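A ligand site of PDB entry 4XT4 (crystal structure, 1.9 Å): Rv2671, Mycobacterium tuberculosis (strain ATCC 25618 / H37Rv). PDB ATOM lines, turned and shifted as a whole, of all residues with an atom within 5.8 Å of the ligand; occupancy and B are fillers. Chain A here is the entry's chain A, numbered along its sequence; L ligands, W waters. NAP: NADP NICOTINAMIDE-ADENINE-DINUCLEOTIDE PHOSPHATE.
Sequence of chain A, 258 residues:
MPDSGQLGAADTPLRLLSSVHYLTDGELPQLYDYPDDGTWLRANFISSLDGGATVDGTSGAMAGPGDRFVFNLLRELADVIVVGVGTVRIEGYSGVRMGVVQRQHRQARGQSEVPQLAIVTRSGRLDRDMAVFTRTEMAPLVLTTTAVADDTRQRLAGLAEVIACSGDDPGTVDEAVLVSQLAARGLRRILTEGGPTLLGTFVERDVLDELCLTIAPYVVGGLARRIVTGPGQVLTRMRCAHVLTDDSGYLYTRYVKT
Water W1 bridges NH1 of Arg 89 (2.5 Å) and O2X of the ligand (2.7 Å).
O2X of the ligand is in hydrogen-bond range of OG1 of Thr 121, 2.9 Å away. The side-chain hydroxyl (OG1) of Thr 197 sits at hydrogen-bond distance from an oxygen (O1N) of the ligand. An oxygen (O5B) of the ligand sits at hydrogen-bond distance from the backbone NH (N) of Gly 86 (3.1 Å). The side-chain hydroxyl of Thr 201 sits at hydrogen-bond distance from a nitrogen (N6A) of the ligand, 2.9 Å away. O1X of the ligand lies within hydrogen-bond range of N of Arg 122, at 2.8 Å. An oxygen (O1A) of the ligand lies within hydrogen-bond range of the backbone NH of Leu 198 (3.0 Å). The side-chain carboxylate (OE2) of Glu 175 lies within hydrogen-bond range of a nitrogen (N6A) of the ligand (2.5 Å). The backbone NH (N) of Ser 123 sits at hydrogen-bond distance from an oxygen (O1X) of the ligand, 2.9 Å away. The side-chain hydroxyl (OG) of Ser 123 is in hydrogen-bond range of an oxygen (O2X) of the ligand (2.7 Å). The backbone NH (N) of Thr 87 lies within hydrogen-bond range of an oxygen (O2A) of the ligand. The backbone NH (N) of Thr 197 sits at hydrogen-bond distance from an oxygen (O1N) of the ligand, 3.1 Å away. The backbone NH (N) of Val 85 is in hydrogen-bond range of an oxygen (O4B) of the ligand, at 3.1 Å. The backbone NH (N) of Gly 195 is in hydrogen-bond range of an oxygen (O2A) of the ligand (2.8 Å).
N of Val 120 lies within hydrogen-bond range of O of Val 83 (2.9 Å). O of Pro 196 lies within hydrogen-bond range of N of Thr 229 (3.2 Å). The side-chain hydroxyl (OG) of Ser 123 sits at hydrogen-bond distance from the backbone NH (N) of Arg 125 (3.0 Å). N of Thr 121 is in hydrogen-bond range of O of Leu 143 (3.0 Å). OG1 of Thr 121 sits at hydrogen-bond distance from OG of Ser 123. The backbone NH (N) of Gly 84 lies within hydrogen-bond range of the backbone carbonyl oxygen (O) of Gly 194, at 2.8 Å. N of Val 85 is in hydrogen-bond range of O of Val 120, 3.1 Å away. The side-chain hydroxyl of Thr 121 is in hydrogen-bond range of the backbone NH of Gly 124 (2.7 Å).
O2A of the ligand sits close to O of Gly 84 (3.4 Å). O4B of the ligand sits close to O of Val 120, 3.5 Å away. Val 173 touches the ligand. C of Gly 194 touches O2A of the ligand, at 3.8 Å. Pro 196 touches the ligand (CD to O2N, 3.4 Å). Hydrophobic or aromatic side chains within 4 Å of the ligand: Val 85, Val 120, Val 173, Pro 196 and Leu 198. Within 4 Å of the ligand: Gly 84, Val 85, Gly 86, Thr 87, Val 120, Thr 121, Arg 122, Ser 123, Val 173, Glu 175, Gly 194, Gly 195, Pro 196, Thr 197, Leu 198 and Thr 201.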
ATOM      1  N   VAL A  83     -10.405   9.575  29.066  1.00  0.00           N
ATOM      2  CA  VAL A  83     -11.429  10.079  28.165  1.00  0.00           C
ATOM      3  C   VAL A  83     -11.320   9.434  26.782  1.00  0.00           C
ATOM      4  O   VAL A  83     -10.226   9.142  26.306  1.00  0.00           O
ATOM      5  CB  VAL A  83     -11.361  11.606  28.037  1.00  0.00           C
ATOM      6  CG1 VAL A  83     -11.903  12.249  29.308  1.00  0.00           C
ATOM      7  CG2 VAL A  83      -9.921  12.079  27.784  1.00  0.00           C
ATOM      8  N   GLY A  84     -12.466   9.204  26.144  1.00  0.00           N
ATOM      9  CA  GLY A  84     -12.483   8.620  24.818  1.00  0.00           C
ATOM     10  C   GLY A  84     -12.091   9.666  23.801  1.00  0.00           C
ATOM     11  O   GLY A  84     -12.150  10.863  24.079  1.00  0.00           O
ATOM     12  N   VAL A  85     -11.687   9.230  22.611  1.00  0.00           N
ATOM     13  CA  VAL A  85     -11.168  10.182  21.628  1.00  0.00           C
ATOM     14  C   VAL A  85     -12.288  11.113  21.112  1.00  0.00           C
ATOM     15  O   VAL A  85     -12.036  12.285  20.776  1.00  0.00           O
ATOM     16  CB  VAL A  85     -10.453   9.463  20.469  1.00  0.00           C
ATOM     17  CG1 VAL A  85     -11.282   8.339  19.958  1.00  0.00           C
ATOM     18  CG2 VAL A  85     -10.181  10.430  19.349  1.00  0.00           C
ATOM     19  N   GLY A  86     -13.507  10.609  21.093  1.00  0.00           N
ATOM     20  CA  GLY A  86     -14.651  11.401  20.644  1.00  0.00           C
ATOM     21  C   GLY A  86     -14.911  12.611  21.519  1.00  0.00           C
ATOM     22  O   GLY A  86     -15.095  13.723  21.025  1.00  0.00           O
ATOM     23  N   THR A  87     -14.913  12.401  22.834  1.00  0.00           N
ATOM     24  CA  THR A  87     -15.199  13.501  23.759  1.00  0.00           C
ATOM     25  C   THR A  87     -14.034  14.508  23.741  1.00  0.00           C
ATOM     26  O   THR A  87     -14.256  15.721  23.871  1.00  0.00           O
ATOM     27  CB  THR A  87     -15.520  12.982  25.186  1.00  0.00           C
ATOM     28  OG1 THR A  87     -16.213  13.992  25.918  1.00  0.00           O
ATOM     29  CG2 THR A  87     -14.261  12.608  25.939  1.00  0.00           C
ATOM     30  N   VAL A  88     -12.816  14.007  23.546  1.00  0.00           N
ATOM     31  CA  VAL A  88     -11.633  14.856  23.403  1.00  0.00           C
ATOM     32  C   VAL A  88     -11.778  15.753  22.179  1.00  0.00           C
ATOM     33  O   VAL A  88     -11.413  16.937  22.222  1.00  0.00           O
ATOM     34  CB  VAL A  88     -10.346  14.015  23.296  1.00  0.00           C
ATOM     35  CG1 VAL A  88      -9.200  14.834  22.707  1.00  0.00           C
ATOM     36  CG2 VAL A  88      -9.954  13.479  24.642  1.00  0.00           C
ATOM     37  N   ARG A  89     -12.299  15.195  21.097  1.00  0.00           N
ATOM     38  CA  ARG A  89     -12.496  15.982  19.881  1.00  0.00           C
ATOM     39  C   ARG A  89     -13.633  16.997  20.025  1.00  0.00           C
ATOM     40  O   ARG A  89     -13.552  18.124  19.536  1.00  0.00           O
ATOM     41  CB  ARG A  89     -12.758  15.072  18.692  1.00  0.00           C
ATOM     42  CG  ARG A  89     -11.542  14.288  18.230  1.00  0.00           C
ATOM     43  CD  ARG A  89     -11.884  13.280  17.139  1.00  0.00           C
ATOM     44  NE  ARG A  89     -10.660  12.762  16.525  1.00  0.00           N
ATOM     45  CZ  ARG A  89     -10.461  11.490  16.162  1.00  0.00           C
ATOM     46  NH1 ARG A  89     -11.420  10.581  16.350  1.00  0.00           N
ATOM     47  NH2 ARG A  89      -9.308  11.139  15.618  1.00  0.00           N
ATOM     48  N   ILE A  90     -14.681  16.584  20.725  1.00  0.00           N
ATOM     49  CA  ILE A  90     -15.905  17.357  20.767  1.00  0.00           C
ATOM     50  C   ILE A  90     -16.005  18.353  21.935  1.00  0.00           C
ATOM     51  O   ILE A  90     -16.471  19.467  21.741  1.00  0.00           O
ATOM     52  CB  ILE A  90     -17.138  16.438  20.680  1.00  0.00           C
ATOM     53  CG1 ILE A  90     -17.001  15.523  19.460  1.00  0.00           C
ATOM     54  CG2 ILE A  90     -18.416  17.253  20.587  1.00  0.00           C
ATOM     55  CD1 ILE A  90     -18.062  14.443  19.372  1.00  0.00           C
ATOM     56  N   VAL A 120      -8.486   7.181  25.134  1.00  0.00           N
ATOM     57  CA  VAL A 120      -8.762   5.825  24.670  1.00  0.00           C
ATOM     58  C   VAL A 120      -9.164   5.811  23.198  1.00  0.00           C
ATOM     59  O   VAL A 120     -10.042   6.568  22.778  1.00  0.00           O
ATOM     60  CB  VAL A 120      -9.899   5.182  25.493  1.00  0.00           C
ATOM     61  CG1 VAL A 120     -10.064   3.706  25.112  1.00  0.00           C
ATOM     62  CG2 VAL A 120      -9.606   5.310  26.977  1.00  0.00           C
ATOM     63  N   THR A 121      -8.526   4.954  22.416  1.00  0.00           N
ATOM     64  CA  THR A 121      -8.839   4.815  21.007  1.00  0.00           C
ATOM     65  C   THR A 121      -8.578   3.389  20.549  1.00  0.00           C
ATOM     66  O   THR A 121      -7.479   2.856  20.735  1.00  0.00           O
ATOM     67  CB  THR A 121      -8.035   5.817  20.134  1.00  0.00           C
ATOM     68  OG1 THR A 121      -8.075   5.412  18.762  1.00  0.00           O
ATOM     69  CG2 THR A 121      -6.565   5.893  20.594  1.00  0.00           C
ATOM     70  N   ARG A 122      -9.570   2.737  19.968  1.00  0.00           N
ATOM     71  CA  ARG A 122      -9.356   1.389  19.460  1.00  0.00           C
ATOM     72  C   ARG A 122      -8.575   1.465  18.156  1.00  0.00           C
ATOM     73  O   ARG A 122      -7.701   0.642  17.891  1.00  0.00           O
ATOM     74  CB  ARG A 122     -10.669   0.652  19.212  1.00  0.00           C
ATOM     75  CG  ARG A 122     -10.441  -0.795  18.770  1.00  0.00           C
ATOM     76  CD  ARG A 122     -11.729  -1.481  18.333  1.00  0.00           C
ATOM     77  NE  ARG A 122     -12.169  -1.061  17.007  1.00  0.00           N
ATOM     78  CZ  ARG A 122     -13.358  -1.369  16.482  1.00  0.00           C
ATOM     79  NH1 ARG A 122     -14.217  -2.093  17.180  1.00  0.00           N
ATOM     80  NH2 ARG A 122     -13.675  -0.959  15.261  1.00  0.00           N
ATOM     81  N   SER A 123      -8.887   2.489  17.354  1.00  0.00           N
ATOM     82  CA  SER A 123      -8.266   2.643  16.052  1.00  0.00           C
ATOM     83  C   SER A 123      -6.810   3.091  16.157  1.00  0.00           C
ATOM     84  O   SER A 123      -5.951   2.654  15.378  1.00  0.00           O
ATOM     85  CB  SER A 123      -9.073   3.618  15.192  1.00  0.00           C
ATOM     86  OG  SER A 123      -8.916   4.947  15.663  1.00  0.00           O
ATOM     87  N   GLY A 124      -6.529   3.970  17.105  1.00  0.00           N
ATOM     88  CA  GLY A 124      -5.216   4.560  17.216  1.00  0.00           C
ATOM     89  C   GLY A 124      -5.065   5.780  16.320  1.00  0.00           C
ATOM     90  O   GLY A 124      -3.999   6.402  16.268  1.00  0.00           O
ATOM     91  N   ARG A 125      -6.125   6.126  15.604  1.00  0.00           N
ATOM     92  CA  ARG A 125      -6.052   7.229  14.646  1.00  0.00           C
ATOM     93  C   ARG A 125      -6.230   8.605  15.292  1.00  0.00           C
ATOM     94  O   ARG A 125      -7.326   9.160  15.318  1.00  0.00           O
ATOM     95  CB  ARG A 125      -7.051   7.014  13.518  1.00  0.00           C
ATOM     96  CG  ARG A 125      -6.857   5.676  12.862  1.00  0.00           C
ATOM     97  CD  ARG A 125      -7.867   5.369  11.789  1.00  0.00           C
ATOM     98  NE  ARG A 125      -7.906   3.937  11.541  1.00  0.00           N
ATOM     99  CZ  ARG A 125      -8.510   3.356  10.506  1.00  0.00           C
ATOM    100  NH1 ARG A 125      -9.122   4.099   9.592  1.00  0.00           N
ATOM    101  NH2 ARG A 125      -8.487   2.047  10.380  1.00  0.00           N
ATOM    102  N   LEU A 143      -4.238   5.150  25.169  1.00  0.00           N
ATOM    103  CA  LEU A 143      -4.550   3.769  25.487  1.00  0.00           C
ATOM    104  C   LEU A 143      -5.197   3.113  24.275  1.00  0.00           C
ATOM    105  O   LEU A 143      -6.285   3.506  23.878  1.00  0.00           O
ATOM    106  CB  LEU A 143      -5.498   3.729  26.689  1.00  0.00           C
ATOM    107  CG  LEU A 143      -5.022   4.615  27.862  1.00  0.00           C
ATOM    108  CD1 LEU A 143      -5.943   4.453  29.065  1.00  0.00           C
ATOM    109  CD2 LEU A 143      -3.560   4.313  28.255  1.00  0.00           C
ATOM    110  N   VAL A 173      -9.577  -3.274  22.809  1.00  0.00           N
ATOM    111  CA  VAL A 173      -9.193  -2.842  24.152  1.00  0.00           C
ATOM    112  C   VAL A 173     -10.008  -3.644  25.169  1.00  0.00           C
ATOM    113  O   VAL A 173     -11.228  -3.740  25.044  1.00  0.00           O
ATOM    114  CB  VAL A 173      -9.450  -1.336  24.351  1.00  0.00           C
ATOM    115  CG1 VAL A 173      -9.264  -0.948  25.810  1.00  0.00           C
ATOM    116  CG2 VAL A 173      -8.542  -0.517  23.464  1.00  0.00           C
ATOM    117  N   GLU A 175     -11.126  -3.505  28.867  1.00  0.00           N
ATOM    118  CA  GLU A 175     -11.209  -2.371  29.803  1.00  0.00           C
ATOM    119  C   GLU A 175     -10.607  -2.665  31.178  1.00  0.00           C
ATOM    120  O   GLU A 175     -10.105  -1.760  31.861  1.00  0.00           O
ATOM    121  CB  GLU A 175     -12.656  -1.884  29.930  1.00  0.00           C
ATOM    122  CG  GLU A 175     -13.166  -1.161  28.680  1.00  0.00           C
ATOM    123  CD  GLU A 175     -13.598  -2.112  27.575  1.00  0.00           C
ATOM    124  OE1 GLU A 175     -13.731  -3.325  27.860  1.00  0.00           O
ATOM    125  OE2 GLU A 175     -13.800  -1.643  26.432  1.00  0.00           O
ATOM    126  N   GLY A 194     -15.902  10.330  30.276  1.00  0.00           N
ATOM    127  CA  GLY A 194     -16.649   9.929  29.092  1.00  0.00           C
ATOM    128  C   GLY A 194     -15.758   9.782  27.866  1.00  0.00           C
ATOM    129  O   GLY A 194     -14.541   9.589  28.004  1.00  0.00           O
ATOM    130  N   GLY A 195     -16.345   9.870  26.668  1.00  0.00           N
ATOM    131  CA  GLY A 195     -17.757  10.161  26.495  1.00  0.00           C
ATOM    132  C   GLY A 195     -18.668   8.970  26.683  1.00  0.00           C
ATOM    133  O   GLY A 195     -18.302   7.988  27.340  1.00  0.00           O
ATOM    134  N   PRO A 196     -19.883   9.041  26.112  1.00  0.00           N
ATOM    135  CA  PRO A 196     -20.896   8.005  26.333  1.00  0.00           C
ATOM    136  C   PRO A 196     -20.505   6.621  25.823  1.00  0.00           C
ATOM    137  O   PRO A 196     -20.919   5.631  26.443  1.00  0.00           O
ATOM    138  CB  PRO A 196     -22.134   8.542  25.569  1.00  0.00           C
ATOM    139  CG  PRO A 196     -21.585   9.529  24.587  1.00  0.00           C
ATOM    140  CD  PRO A 196     -20.404  10.148  25.289  1.00  0.00           C
ATOM    141  N   THR A 197     -19.752   6.527  24.728  1.00  0.00           N
ATOM    142  CA  THR A 197     -19.345   5.196  24.266  1.00  0.00           C
ATOM    143  C   THR A 197     -18.388   4.532  25.261  1.00  0.00           C
ATOM    144  O   THR A 197     -18.577   3.376  25.645  1.00  0.00           O
ATOM    145  CB  THR A 197     -18.694   5.248  22.866  1.00  0.00           C
ATOM    146  OG1 THR A 197     -19.610   5.883  21.950  1.00  0.00           O
ATOM    147  CG2 THR A 197     -18.387   3.830  22.365  1.00  0.00           C
ATOM    148  N   LEU A 198     -17.347   5.263  25.677  1.00  0.00           N
ATOM    149  CA  LEU A 198     -16.399   4.726  26.660  1.00  0.00           C
ATOM    150  C   LEU A 198     -17.094   4.352  27.968  1.00  0.00           C
ATOM    151  O   LEU A 198     -16.909   3.245  28.482  1.00  0.00           O
ATOM    152  CB  LEU A 198     -15.266   5.723  26.913  1.00  0.00           C
ATOM    153  CG  LEU A 198     -14.223   5.257  27.929  1.00  0.00           C
ATOM    154  CD1 LEU A 198     -13.495   4.031  27.428  1.00  0.00           C
ATOM    155  CD2 LEU A 198     -13.240   6.369  28.225  1.00  0.00           C
ATOM    156  N   LEU A 199     -17.889   5.274  28.528  1.00  0.00           N
ATOM    157  CA  LEU A 199     -18.620   4.942  29.753  1.00  0.00           C
ATOM    158  C   LEU A 199     -19.462   3.687  29.534  1.00  0.00           C
ATOM    159  O   LEU A 199     -19.519   2.790  30.398  1.00  0.00           O
ATOM    160  CB  LEU A 199     -19.500   6.105  30.219  1.00  0.00           C
ATOM    161  CG  LEU A 199     -20.302   5.859  31.506  1.00  0.00           C
ATOM    162  CD1 LEU A 199     -19.400   5.539  32.670  1.00  0.00           C
ATOM    163  CD2 LEU A 199     -21.206   7.050  31.861  1.00  0.00           C
ATOM    164  N   THR A 201     -18.815   1.205  27.634  1.00  0.00           N
ATOM    165  CA  THR A 201     -17.986  -0.006  27.718  1.00  0.00           C
ATOM    166  C   THR A 201     -17.525  -0.315  29.139  1.00  0.00           C
ATOM    167  O   THR A 201     -17.393  -1.491  29.516  1.00  0.00           O
ATOM    168  CB  THR A 201     -16.756   0.083  26.802  1.00  0.00           C
ATOM    169  OG1 THR A 201     -15.875   1.115  27.264  1.00  0.00           O
ATOM    170  CG2 THR A 201     -17.185   0.393  25.380  1.00  0.00           C
ATOM    171  N   ARG A 225     -28.870  12.603  23.839  1.00  0.00           N
ATOM    172  CA  ARG A 225     -28.463  11.244  24.180  1.00  0.00           C
ATOM    173  C   ARG A 225     -28.321  11.134  25.685  1.00  0.00           C
ATOM    174  O   ARG A 225     -28.270  12.141  26.385  1.00  0.00           O
ATOM    175  CB  ARG A 225     -27.112  10.939  23.530  1.00  0.00           C
ATOM    176  CG  ARG A 225     -26.001  11.862  24.010  1.00  0.00           C
ATOM    177  CD  ARG A 225     -24.606  11.397  23.577  1.00  0.00           C
ATOM    178  NE  ARG A 225     -23.572  12.390  23.894  1.00  0.00           N
ATOM    179  CZ  ARG A 225     -23.039  12.573  25.105  1.00  0.00           C
ATOM    180  NH1 ARG A 225     -23.459  11.843  26.133  1.00  0.00           N
ATOM    181  NH2 ARG A 225     -22.085  13.486  25.288  1.00  0.00           N
ATOM    182  N   THR A 229     -23.998   5.388  25.795  1.00  0.00           N
ATOM    183  CA  THR A 229     -24.561   4.913  24.536  1.00  0.00           C
ATOM    184  C   THR A 229     -23.913   3.577  24.178  1.00  0.00           C
ATOM    185  O   THR A 229     -22.915   3.168  24.796  1.00  0.00           O
ATOM    186  CB  THR A 229     -24.358   5.905  23.369  1.00  0.00           C
ATOM    187  OG1 THR A 229     -22.953   6.160  23.194  1.00  0.00           O
ATOM    188  CG2 THR A 229     -25.063   7.229  23.648  1.00  0.00           C
HETATM  189  PA  NAP L   1     -16.304   8.945  23.313  1.00  0.00           P
HETATM  190  O1A NAP L   1     -16.638   7.716  24.087  1.00  0.00           O
HETATM  191  O2A NAP L   1     -15.336   9.796  24.100  1.00  0.00           O
HETATM  192  O5B NAP L   1     -15.745   8.581  21.927  1.00  0.00           O
HETATM  193  C5B NAP L   1     -15.743   7.289  21.467  1.00  0.00           C
HETATM  194  C4B NAP L   1     -14.447   6.851  20.822  1.00  0.00           C
HETATM  195  O4B NAP L   1     -13.363   6.707  21.805  1.00  0.00           O
HETATM  196  C3B NAP L   1     -14.527   5.556  20.094  1.00  0.00           C
HETATM  197  O3B NAP L   1     -14.784   5.701  18.745  1.00  0.00           O
HETATM  198  C2B NAP L   1     -13.201   4.993  20.265  1.00  0.00           C
HETATM  199  O2B NAP L   1     -12.263   5.531  19.409  1.00  0.00           O
HETATM  200  C1B NAP L   1     -12.900   5.410  21.685  1.00  0.00           C
HETATM  201  N9A NAP L   1     -13.411   4.466  22.686  1.00  0.00           N
HETATM  202  C8A NAP L   1     -14.431   4.599  23.554  1.00  0.00           C
HETATM  203  N7A NAP L   1     -14.516   3.460  24.263  1.00  0.00           N
HETATM  204  C5A NAP L   1     -13.557   2.602  23.852  1.00  0.00           C
HETATM  205  C6A NAP L   1     -13.149   1.322  24.193  1.00  0.00           C
HETATM  206  N6A NAP L   1     -13.806   0.541  25.245  1.00  0.00           N
HETATM  207  N1A NAP L   1     -12.106   0.785  23.543  1.00  0.00           N
HETATM  208  C2A NAP L   1     -11.442   1.432  22.567  1.00  0.00           C
HETATM  209  N3A NAP L   1     -11.822   2.666  22.217  1.00  0.00           N
HETATM  210  C4A NAP L   1     -12.856   3.259  22.852  1.00  0.00           C
HETATM  211  O3  NAP L   1     -17.594   9.812  23.093  1.00  0.00           O
HETATM  212  PN  NAP L   1     -18.660   9.606  21.983  1.00  0.00           P
HETATM  213  O1N NAP L   1     -19.406   8.330  22.172  1.00  0.00           O
HETATM  214  O2N NAP L   1     -19.633  10.842  22.059  1.00  0.00           O
HETATM  215  O5D NAP L   1     -18.040   9.606  20.606  1.00  0.00           O
HETATM  216  P2B NAP L   1     -11.896   4.990  17.998  1.00  0.00           P
HETATM  217  O1X NAP L   1     -11.518   3.544  18.052  1.00  0.00           O
HETATM  218  O2X NAP L   1     -10.703   5.800  17.515  1.00  0.00           O
HETATM  219  O3X NAP L   1     -13.047   5.205  17.059  1.00  0.00           O
HETATM  220  O   HOH W   1     -10.759   8.148  16.265  1.00  0.00           O
